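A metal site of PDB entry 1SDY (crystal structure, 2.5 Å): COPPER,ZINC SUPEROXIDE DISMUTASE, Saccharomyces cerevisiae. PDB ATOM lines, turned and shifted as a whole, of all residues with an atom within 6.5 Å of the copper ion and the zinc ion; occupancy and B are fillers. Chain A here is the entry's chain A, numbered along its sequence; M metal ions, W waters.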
ATOM      1  N   GLY A  44       5.196  32.365  20.518  1.00  0.00           N
ATOM      2  CA  GLY A  44       4.539  31.404  21.409  1.00  0.00           C
ATOM      3  C   GLY A  44       3.428  31.976  22.256  1.00  0.00           C
ATOM      4  O   GLY A  44       3.565  33.066  22.779  1.00  0.00           O
ATOM      5  N   PHE A  45       2.320  31.239  22.406  1.00  0.00           N
ATOM      6  CA  PHE A  45       1.158  31.777  23.094  1.00  0.00           C
ATOM      7  C   PHE A  45       0.598  30.681  23.940  1.00  0.00           C
ATOM      8  O   PHE A  45       0.021  29.736  23.423  1.00  0.00           O
ATOM      9  CB  PHE A  45       0.171  32.216  21.990  1.00  0.00           C
ATOM     10  CG  PHE A  45      -1.106  32.862  22.406  1.00  0.00           C
ATOM     11  CD1 PHE A  45      -1.060  34.022  23.185  1.00  0.00           C
ATOM     12  CD2 PHE A  45      -2.319  32.399  21.897  1.00  0.00           C
ATOM     13  CE1 PHE A  45      -2.227  34.734  23.473  1.00  0.00           C
ATOM     14  CE2 PHE A  45      -3.494  33.109  22.156  1.00  0.00           C
ATOM     15  CZ  PHE A  45      -3.428  34.277  22.915  1.00  0.00           C
ATOM     16  N   HIS A  46       0.699  30.928  25.234  1.00  0.00           N
ATOM     17  CA  HIS A  46       0.329  29.963  26.237  1.00  0.00           C
ATOM     18  C   HIS A  46      -0.380  30.494  27.462  1.00  0.00           C
ATOM     19  O   HIS A  46      -0.325  31.649  27.821  1.00  0.00           O
ATOM     20  CB  HIS A  46       1.667  29.457  26.826  1.00  0.00           C
ATOM     21  CG  HIS A  46       2.710  29.126  25.814  1.00  0.00           C
ATOM     22  ND1 HIS A  46       4.058  29.385  26.056  1.00  0.00           N
ATOM     23  CD2 HIS A  46       2.618  28.502  24.612  1.00  0.00           C
ATOM     24  CE1 HIS A  46       4.744  28.939  25.012  1.00  0.00           C
ATOM     25  NE2 HIS A  46       3.912  28.369  24.133  1.00  0.00           N
ATOM     26  N   ILE A  47      -0.927  29.552  28.176  1.00  0.00           N
ATOM     27  CA  ILE A  47      -1.521  29.734  29.438  1.00  0.00           C
ATOM     28  C   ILE A  47      -0.585  29.080  30.447  1.00  0.00           C
ATOM     29  O   ILE A  47      -0.238  27.892  30.381  1.00  0.00           O
ATOM     30  CB  ILE A  47      -2.934  29.159  29.573  1.00  0.00           C
ATOM     31  CG1 ILE A  47      -3.927  30.065  28.800  1.00  0.00           C
ATOM     32  CG2 ILE A  47      -3.205  29.181  31.079  1.00  0.00           C
ATOM     33  CD1 ILE A  47      -5.194  29.421  28.250  1.00  0.00           C
ATOM     34  N   HIS A  48      -0.093  29.914  31.344  1.00  0.00           N
ATOM     35  CA  HIS A  48       0.814  29.595  32.419  1.00  0.00           C
ATOM     36  C   HIS A  48      -0.085  29.463  33.662  1.00  0.00           C
ATOM     37  O   HIS A  48      -1.198  30.012  33.746  1.00  0.00           O
ATOM     38  CB  HIS A  48       1.916  30.714  32.590  1.00  0.00           C
ATOM     39  CG  HIS A  48       2.962  30.663  31.568  1.00  0.00           C
ATOM     40  ND1 HIS A  48       4.276  30.358  31.924  1.00  0.00           N
ATOM     41  CD2 HIS A  48       2.893  30.801  30.210  1.00  0.00           C
ATOM     42  CE1 HIS A  48       4.970  30.302  30.775  1.00  0.00           C
ATOM     43  NE2 HIS A  48       4.169  30.568  29.735  1.00  0.00           N
ATOM     44  N   GLY A  61       4.638  31.511  36.452  1.00  0.00           N
ATOM     45  CA  GLY A  61       5.065  30.161  36.480  1.00  0.00           C
ATOM     46  C   GLY A  61       5.163  29.474  35.106  1.00  0.00           C
ATOM     47  O   GLY A  61       5.276  30.079  34.021  1.00  0.00           O
ATOM     48  N   PRO A  62       5.073  28.148  35.176  1.00  0.00           N
ATOM     49  CA  PRO A  62       5.232  27.332  34.007  1.00  0.00           C
ATOM     50  C   PRO A  62       3.903  27.200  33.302  1.00  0.00           C
ATOM     51  O   PRO A  62       2.969  27.887  33.635  1.00  0.00           O
ATOM     52  CB  PRO A  62       5.708  25.982  34.540  1.00  0.00           C
ATOM     53  CG  PRO A  62       5.142  25.894  35.978  1.00  0.00           C
ATOM     54  CD  PRO A  62       4.861  27.315  36.434  1.00  0.00           C
ATOM     55  N   HIS A  63       3.830  26.336  32.279  1.00  0.00           N
ATOM     56  CA  HIS A  63       2.594  26.177  31.549  1.00  0.00           C
ATOM     57  C   HIS A  63       1.539  25.436  32.339  1.00  0.00           C
ATOM     58  O   HIS A  63       1.864  24.452  32.986  1.00  0.00           O
ATOM     59  CB  HIS A  63       2.912  25.350  30.314  1.00  0.00           C
ATOM     60  CG  HIS A  63       3.660  26.105  29.278  1.00  0.00           C
ATOM     61  ND1 HIS A  63       4.061  25.465  28.121  1.00  0.00           N
ATOM     62  CD2 HIS A  63       4.044  27.406  29.247  1.00  0.00           C
ATOM     63  CE1 HIS A  63       4.666  26.395  27.405  1.00  0.00           C
ATOM     64  NE2 HIS A  63       4.674  27.572  28.038  1.00  0.00           N
ATOM     65  N   PHE A  64       0.287  25.910  32.372  1.00  0.00           N
ATOM     66  CA  PHE A  64      -0.712  25.177  33.134  1.00  0.00           C
ATOM     67  C   PHE A  64      -0.751  23.780  32.498  1.00  0.00           C
ATOM     68  O   PHE A  64      -0.879  23.670  31.283  1.00  0.00           O
ATOM     69  CB  PHE A  64      -2.038  25.823  32.902  1.00  0.00           C
ATOM     70  CG  PHE A  64      -3.203  25.167  33.567  1.00  0.00           C
ATOM     71  CD1 PHE A  64      -3.140  24.842  34.925  1.00  0.00           C
ATOM     72  CD2 PHE A  64      -4.391  24.915  32.883  1.00  0.00           C
ATOM     73  CE1 PHE A  64      -4.251  24.353  35.601  1.00  0.00           C
ATOM     74  CE2 PHE A  64      -5.502  24.342  33.522  1.00  0.00           C
ATOM     75  CZ  PHE A  64      -5.426  24.086  34.894  1.00  0.00           C
ATOM     76  N   THR A  70       3.794  16.495  28.479  1.00  0.00           N
ATOM     77  CA  THR A  70       4.877  17.323  27.998  1.00  0.00           C
ATOM     78  C   THR A  70       4.293  18.365  27.024  1.00  0.00           C
ATOM     79  O   THR A  70       3.149  18.266  26.472  1.00  0.00           O
ATOM     80  CB  THR A  70       5.999  16.490  27.298  1.00  0.00           C
ATOM     81  OG1 THR A  70       5.444  15.553  26.397  1.00  0.00           O
ATOM     82  CG2 THR A  70       6.867  15.691  28.262  1.00  0.00           C
ATOM     83  N   HIS A  71       5.121  19.347  26.740  1.00  0.00           N
ATOM     84  CA  HIS A  71       4.770  20.415  25.818  1.00  0.00           C
ATOM     85  C   HIS A  71       4.551  19.896  24.379  1.00  0.00           C
ATOM     86  O   HIS A  71       5.196  18.972  23.907  1.00  0.00           O
ATOM     87  CB  HIS A  71       5.852  21.534  25.939  1.00  0.00           C
ATOM     88  CG  HIS A  71       5.536  22.721  25.087  1.00  0.00           C
ATOM     89  ND1 HIS A  71       4.650  23.718  25.505  1.00  0.00           N
ATOM     90  CD2 HIS A  71       5.950  23.030  23.818  1.00  0.00           C
ATOM     91  CE1 HIS A  71       4.562  24.588  24.509  1.00  0.00           C
ATOM     92  NE2 HIS A  71       5.335  24.209  23.479  1.00  0.00           N
ATOM     93  N   GLY A  72       3.604  20.465  23.653  1.00  0.00           N
ATOM     94  CA  GLY A  72       3.284  20.029  22.316  1.00  0.00           C
ATOM     95  C   GLY A  72       2.531  21.163  21.611  1.00  0.00           C
ATOM     96  O   GLY A  72       2.444  22.280  22.116  1.00  0.00           O
ATOM     97  N   ARG A  79       0.197  17.201  25.129  1.00  0.00           N
ATOM     98  CA  ARG A  79       0.445  18.621  25.197  1.00  0.00           C
ATOM     99  C   ARG A  79      -0.035  19.109  26.515  1.00  0.00           C
ATOM    100  O   ARG A  79      -0.908  18.445  27.064  1.00  0.00           O
ATOM    101  CB  ARG A  79      -0.429  19.330  24.159  1.00  0.00           C
ATOM    102  CG  ARG A  79      -1.941  19.108  24.313  1.00  0.00           C
ATOM    103  CD  ARG A  79      -2.715  20.191  23.552  1.00  0.00           C
ATOM    104  NE  ARG A  79      -3.127  21.360  24.349  1.00  0.00           N
ATOM    105  CZ  ARG A  79      -4.179  22.099  23.977  1.00  0.00           C
ATOM    106  NH1 ARG A  79      -4.827  21.813  22.881  1.00  0.00           N
ATOM    107  NH2 ARG A  79      -4.662  23.113  24.708  1.00  0.00           N
ATOM    108  N   HIS A  80       0.437  20.288  26.932  1.00  0.00           N
ATOM    109  CA  HIS A  80      -0.108  20.938  28.112  1.00  0.00           C
ATOM    110  C   HIS A  80      -1.488  21.569  27.758  1.00  0.00           C
ATOM    111  O   HIS A  80      -1.762  21.913  26.604  1.00  0.00           O
ATOM    112  CB  HIS A  80       0.809  22.055  28.526  1.00  0.00           C
ATOM    113  CG  HIS A  80       2.203  21.624  28.811  1.00  0.00           C
ATOM    114  ND1 HIS A  80       3.279  22.458  28.529  1.00  0.00           N
ATOM    115  CD2 HIS A  80       2.653  20.483  29.390  1.00  0.00           C
ATOM    116  CE1 HIS A  80       4.358  21.833  28.957  1.00  0.00           C
ATOM    117  NE2 HIS A  80       3.999  20.670  29.510  1.00  0.00           N
ATOM    118  N   GLY A  82      -2.184  24.359  28.686  1.00  0.00           N
ATOM    119  CA  GLY A  82      -1.916  25.724  28.307  1.00  0.00           C
ATOM    120  C   GLY A  82      -1.356  25.996  26.890  1.00  0.00           C
ATOM    121  O   GLY A  82      -1.273  27.157  26.481  1.00  0.00           O
ATOM    122  N   ASP A  83      -0.881  24.973  26.186  1.00  0.00           N
ATOM    123  CA  ASP A  83      -0.203  25.077  24.899  1.00  0.00           C
ATOM    124  C   ASP A  83      -1.132  25.611  23.777  1.00  0.00           C
ATOM    125  O   ASP A  83      -1.956  24.866  23.248  1.00  0.00           O
ATOM    126  CB  ASP A  83       0.458  23.692  24.552  1.00  0.00           C
ATOM    127  CG  ASP A  83       1.576  23.361  25.511  1.00  0.00           C
ATOM    128  OD1 ASP A  83       2.093  24.287  26.205  1.00  0.00           O
ATOM    129  OD2 ASP A  83       1.982  22.175  25.629  1.00  0.00           O
ATOM    130  N   VAL A 118       0.286  34.225  28.510  1.00  0.00           N
ATOM    131  CA  VAL A 118       1.614  34.620  28.085  1.00  0.00           C
ATOM    132  C   VAL A 118       1.862  34.754  26.583  1.00  0.00           C
ATOM    133  O   VAL A 118       1.537  33.821  25.823  1.00  0.00           O
ATOM    134  CB  VAL A 118       2.761  34.717  29.107  1.00  0.00           C
ATOM    135  CG1 VAL A 118       2.686  33.746  30.292  1.00  0.00           C
ATOM    136  CG2 VAL A 118       4.106  34.599  28.438  1.00  0.00           C
ATOM    137  N   HIS A 120       4.989  35.292  24.113  1.00  0.00           N
ATOM    138  CA  HIS A 120       6.434  35.199  24.180  1.00  0.00           C
ATOM    139  C   HIS A 120       7.170  36.060  23.135  1.00  0.00           C
ATOM    140  O   HIS A 120       6.608  36.489  22.127  1.00  0.00           O
ATOM    141  CB  HIS A 120       6.838  33.734  23.946  1.00  0.00           C
ATOM    142  CG  HIS A 120       6.549  32.949  25.146  1.00  0.00           C
ATOM    143  ND1 HIS A 120       7.438  32.942  26.194  1.00  0.00           N
ATOM    144  CD2 HIS A 120       5.506  32.120  25.428  1.00  0.00           C
ATOM    145  CE1 HIS A 120       6.906  32.166  27.133  1.00  0.00           C
ATOM    146  NE2 HIS A 120       5.731  31.675  26.714  1.00  0.00           N
ATOM    147  N   ASP A 124       7.376  29.162  19.300  1.00  0.00           N
ATOM    148  CA  ASP A 124       7.288  27.942  20.015  1.00  0.00           C
ATOM    149  C   ASP A 124       7.670  26.795  19.085  1.00  0.00           C
ATOM    150  O   ASP A 124       6.983  26.572  18.095  1.00  0.00           O
ATOM    151  CB  ASP A 124       5.840  27.815  20.401  1.00  0.00           C
ATOM    152  CG  ASP A 124       5.573  26.622  21.305  1.00  0.00           C
ATOM    153  OD1 ASP A 124       6.338  25.618  21.271  1.00  0.00           O
ATOM    154  OD2 ASP A 124       4.491  26.660  21.942  1.00  0.00           O
ATOM    155  N   SER A 134      12.562  21.982  25.040  1.00  0.00           N
ATOM    156  CA  SER A 134      11.523  21.971  24.070  1.00  0.00           C
ATOM    157  C   SER A 134      10.270  21.279  24.596  1.00  0.00           C
ATOM    158  O   SER A 134       9.101  21.675  24.399  1.00  0.00           O
ATOM    159  CB  SER A 134      11.960  21.218  22.835  1.00  0.00           C
ATOM    160  OG  SER A 134      10.766  20.700  22.242  1.00  0.00           O
ATOM    161  N   LEU A 135      10.591  20.209  25.283  1.00  0.00           N
ATOM    162  CA  LEU A 135       9.611  19.391  25.929  1.00  0.00           C
ATOM    163  C   LEU A 135       8.929  20.098  27.131  1.00  0.00           C
ATOM    164  O   LEU A 135       7.866  19.663  27.628  1.00  0.00           O
ATOM    165  CB  LEU A 135      10.278  18.061  26.314  1.00  0.00           C
ATOM    166  CG  LEU A 135       9.905  16.935  25.369  1.00  0.00           C
ATOM    167  CD1 LEU A 135       9.474  17.578  24.057  1.00  0.00           C
ATOM    168  CD2 LEU A 135      11.070  15.969  25.166  1.00  0.00           C
ATOM    169  N   LYS A 136       9.527  21.194  27.601  1.00  0.00           N
ATOM    170  CA  LYS A 136       9.016  21.975  28.754  1.00  0.00           C
ATOM    171  C   LYS A 136       8.259  23.258  28.378  1.00  0.00           C
ATOM    172  O   LYS A 136       7.096  23.507  28.798  1.00  0.00           O
ATOM    173  CB  LYS A 136      10.202  22.408  29.579  1.00  0.00           C
ATOM    174  CG  LYS A 136      10.676  21.364  30.589  1.00  0.00           C
ATOM    175  N   THR A 137       8.946  24.028  27.523  1.00  0.00           N
ATOM    176  CA  THR A 137       8.470  25.320  27.039  1.00  0.00           C
ATOM    177  C   THR A 137       8.409  25.552  25.522  1.00  0.00           C
ATOM    178  O   THR A 137       8.016  26.649  25.066  1.00  0.00           O
ATOM    179  CB  THR A 137       9.412  26.381  27.632  1.00  0.00           C
ATOM    180  OG1 THR A 137      10.717  26.313  27.040  1.00  0.00           O
ATOM    181  CG2 THR A 137       9.500  26.061  29.104  1.00  0.00           C
ATOM    182  N   GLY A 138       8.842  24.564  24.723  1.00  0.00           N
ATOM    183  CA  GLY A 138       8.871  24.782  23.261  1.00  0.00           C
ATOM    184  C   GLY A 138       9.891  25.851  22.864  1.00  0.00           C
ATOM    185  O   GLY A 138       9.905  26.343  21.710  1.00  0.00           O
ATOM    186  N   ALA A 140      10.152  28.901  23.716  1.00  0.00           N
ATOM    187  CA  ALA A 140       9.545  30.115  23.268  1.00  0.00           C
ATOM    188  C   ALA A 140      10.263  31.379  23.678  1.00  0.00           C
ATOM    189  O   ALA A 140       9.920  32.472  23.250  1.00  0.00           O
ATOM    190  CB  ALA A 140       8.074  30.145  23.657  1.00  0.00           C
ATOM    191  N   GLY A 141      11.212  31.301  24.582  1.00  0.00           N
ATOM    192  CA  GLY A 141      11.839  32.563  24.922  1.00  0.00           C
ATOM    193  C   GLY A 141      11.148  33.327  26.031  1.00  0.00           C
ATOM    194  O   GLY A 141      10.253  32.809  26.681  1.00  0.00           O
ATOM    195  N   ARG A 143       9.215  36.497  28.176  1.00  0.00           N
ATOM    196  CA  ARG A 143       7.798  36.863  28.155  1.00  0.00           C
ATOM    197  C   ARG A 143       7.568  38.360  28.199  1.00  0.00           C
ATOM    198  O   ARG A 143       7.487  38.931  29.268  1.00  0.00           O
ATOM    199  CB  ARG A 143       7.205  36.300  29.432  1.00  0.00           C
ATOM    200  CG  ARG A 143       7.802  34.946  29.836  1.00  0.00           C
ATOM    201  CD  ARG A 143       7.444  34.485  31.259  1.00  0.00           C
ATOM    202  NE  ARG A 143       7.735  33.072  31.594  1.00  0.00           N
ATOM    203  CZ  ARG A 143       7.241  32.387  32.651  1.00  0.00           C
ATOM    204  NH1 ARG A 143       6.387  32.859  33.592  1.00  0.00           N
ATOM    205  NH2 ARG A 143       7.621  31.120  32.717  1.00  0.00           N
HETATM  206 CU    CU M   1       4.655  29.987  27.702  1.00  0.00          CU
HETATM  207 ZN    ZN M   2       3.646  23.859  27.114  1.00  0.00          ZN
HETATM  208  O   HOH W   1       6.349  29.546  28.303  1.00  0.00           O
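OD2 of Asp 83 lies within hydrogen-bond range of N of Gly 72, at 3.1 Å. NE2 of His 71 sits at hydrogen-bond distance from OD1 of Asp 124, 2.8 Å away. N of His 120 lies within hydrogen-bond range of O of Gly 44 (3.0 Å). O of Leu 135 lies within hydrogen-bond range of N of His 71. ND1 of His 120 lies within hydrogen-bond range of O of Gly 141. O of Pro 62 lies close to ND1 of His 48 (3.3 Å). The backbone NH (N) of His 80 lies within hydrogen-bond range of the backbone carbonyl oxygen (O) of Thr 70 (3.4 Å). A ring nitrogen (NE2) of His 46 is in hydrogen-bond range of the side-chain carboxylate (OD2) of Asp 124, at 2.8 Å.
Of the 27 residues printed, 4 come within 4 Å of the copper ion. The nearest printed residue that does not touch the copper ion is Val 118 (4.7 Å).
Lys 136 touches the zinc ion (O to ZN, 3.9 Å). Within 4 Å of the zinc ion: His 63, His 71, His 80, Asp 83 and Lys 136. The nearest printed residue that does not touch the zinc ion is Gly 72 (4.8 Å).
The copper ion is bound by a ring nitrogen (ND1) of His 46 (1.9 Å). The copper ion is bound by water W1 (1.9 Å). A ring nitrogen (NE2) of His 48 binds the copper ion (2.2 Å). NE2 of His 120 binds the copper ion. NE2 of His 63 binds the copper ion. The copper ion has five donor atoms within binding distance.
The zinc ion is bound by OD1 of Asp 83 (1.8 Å), ND1 of His 71 (1.9 Å), ND1 of His 63 (1.9 Å) and ND1 of His 80 (2.0 Å). The zinc ion has four donor atoms within binding distance. Slightly farther from the zinc ion lies the side-chain carboxylate (OD2) of Asp 83 (2.8 Å).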
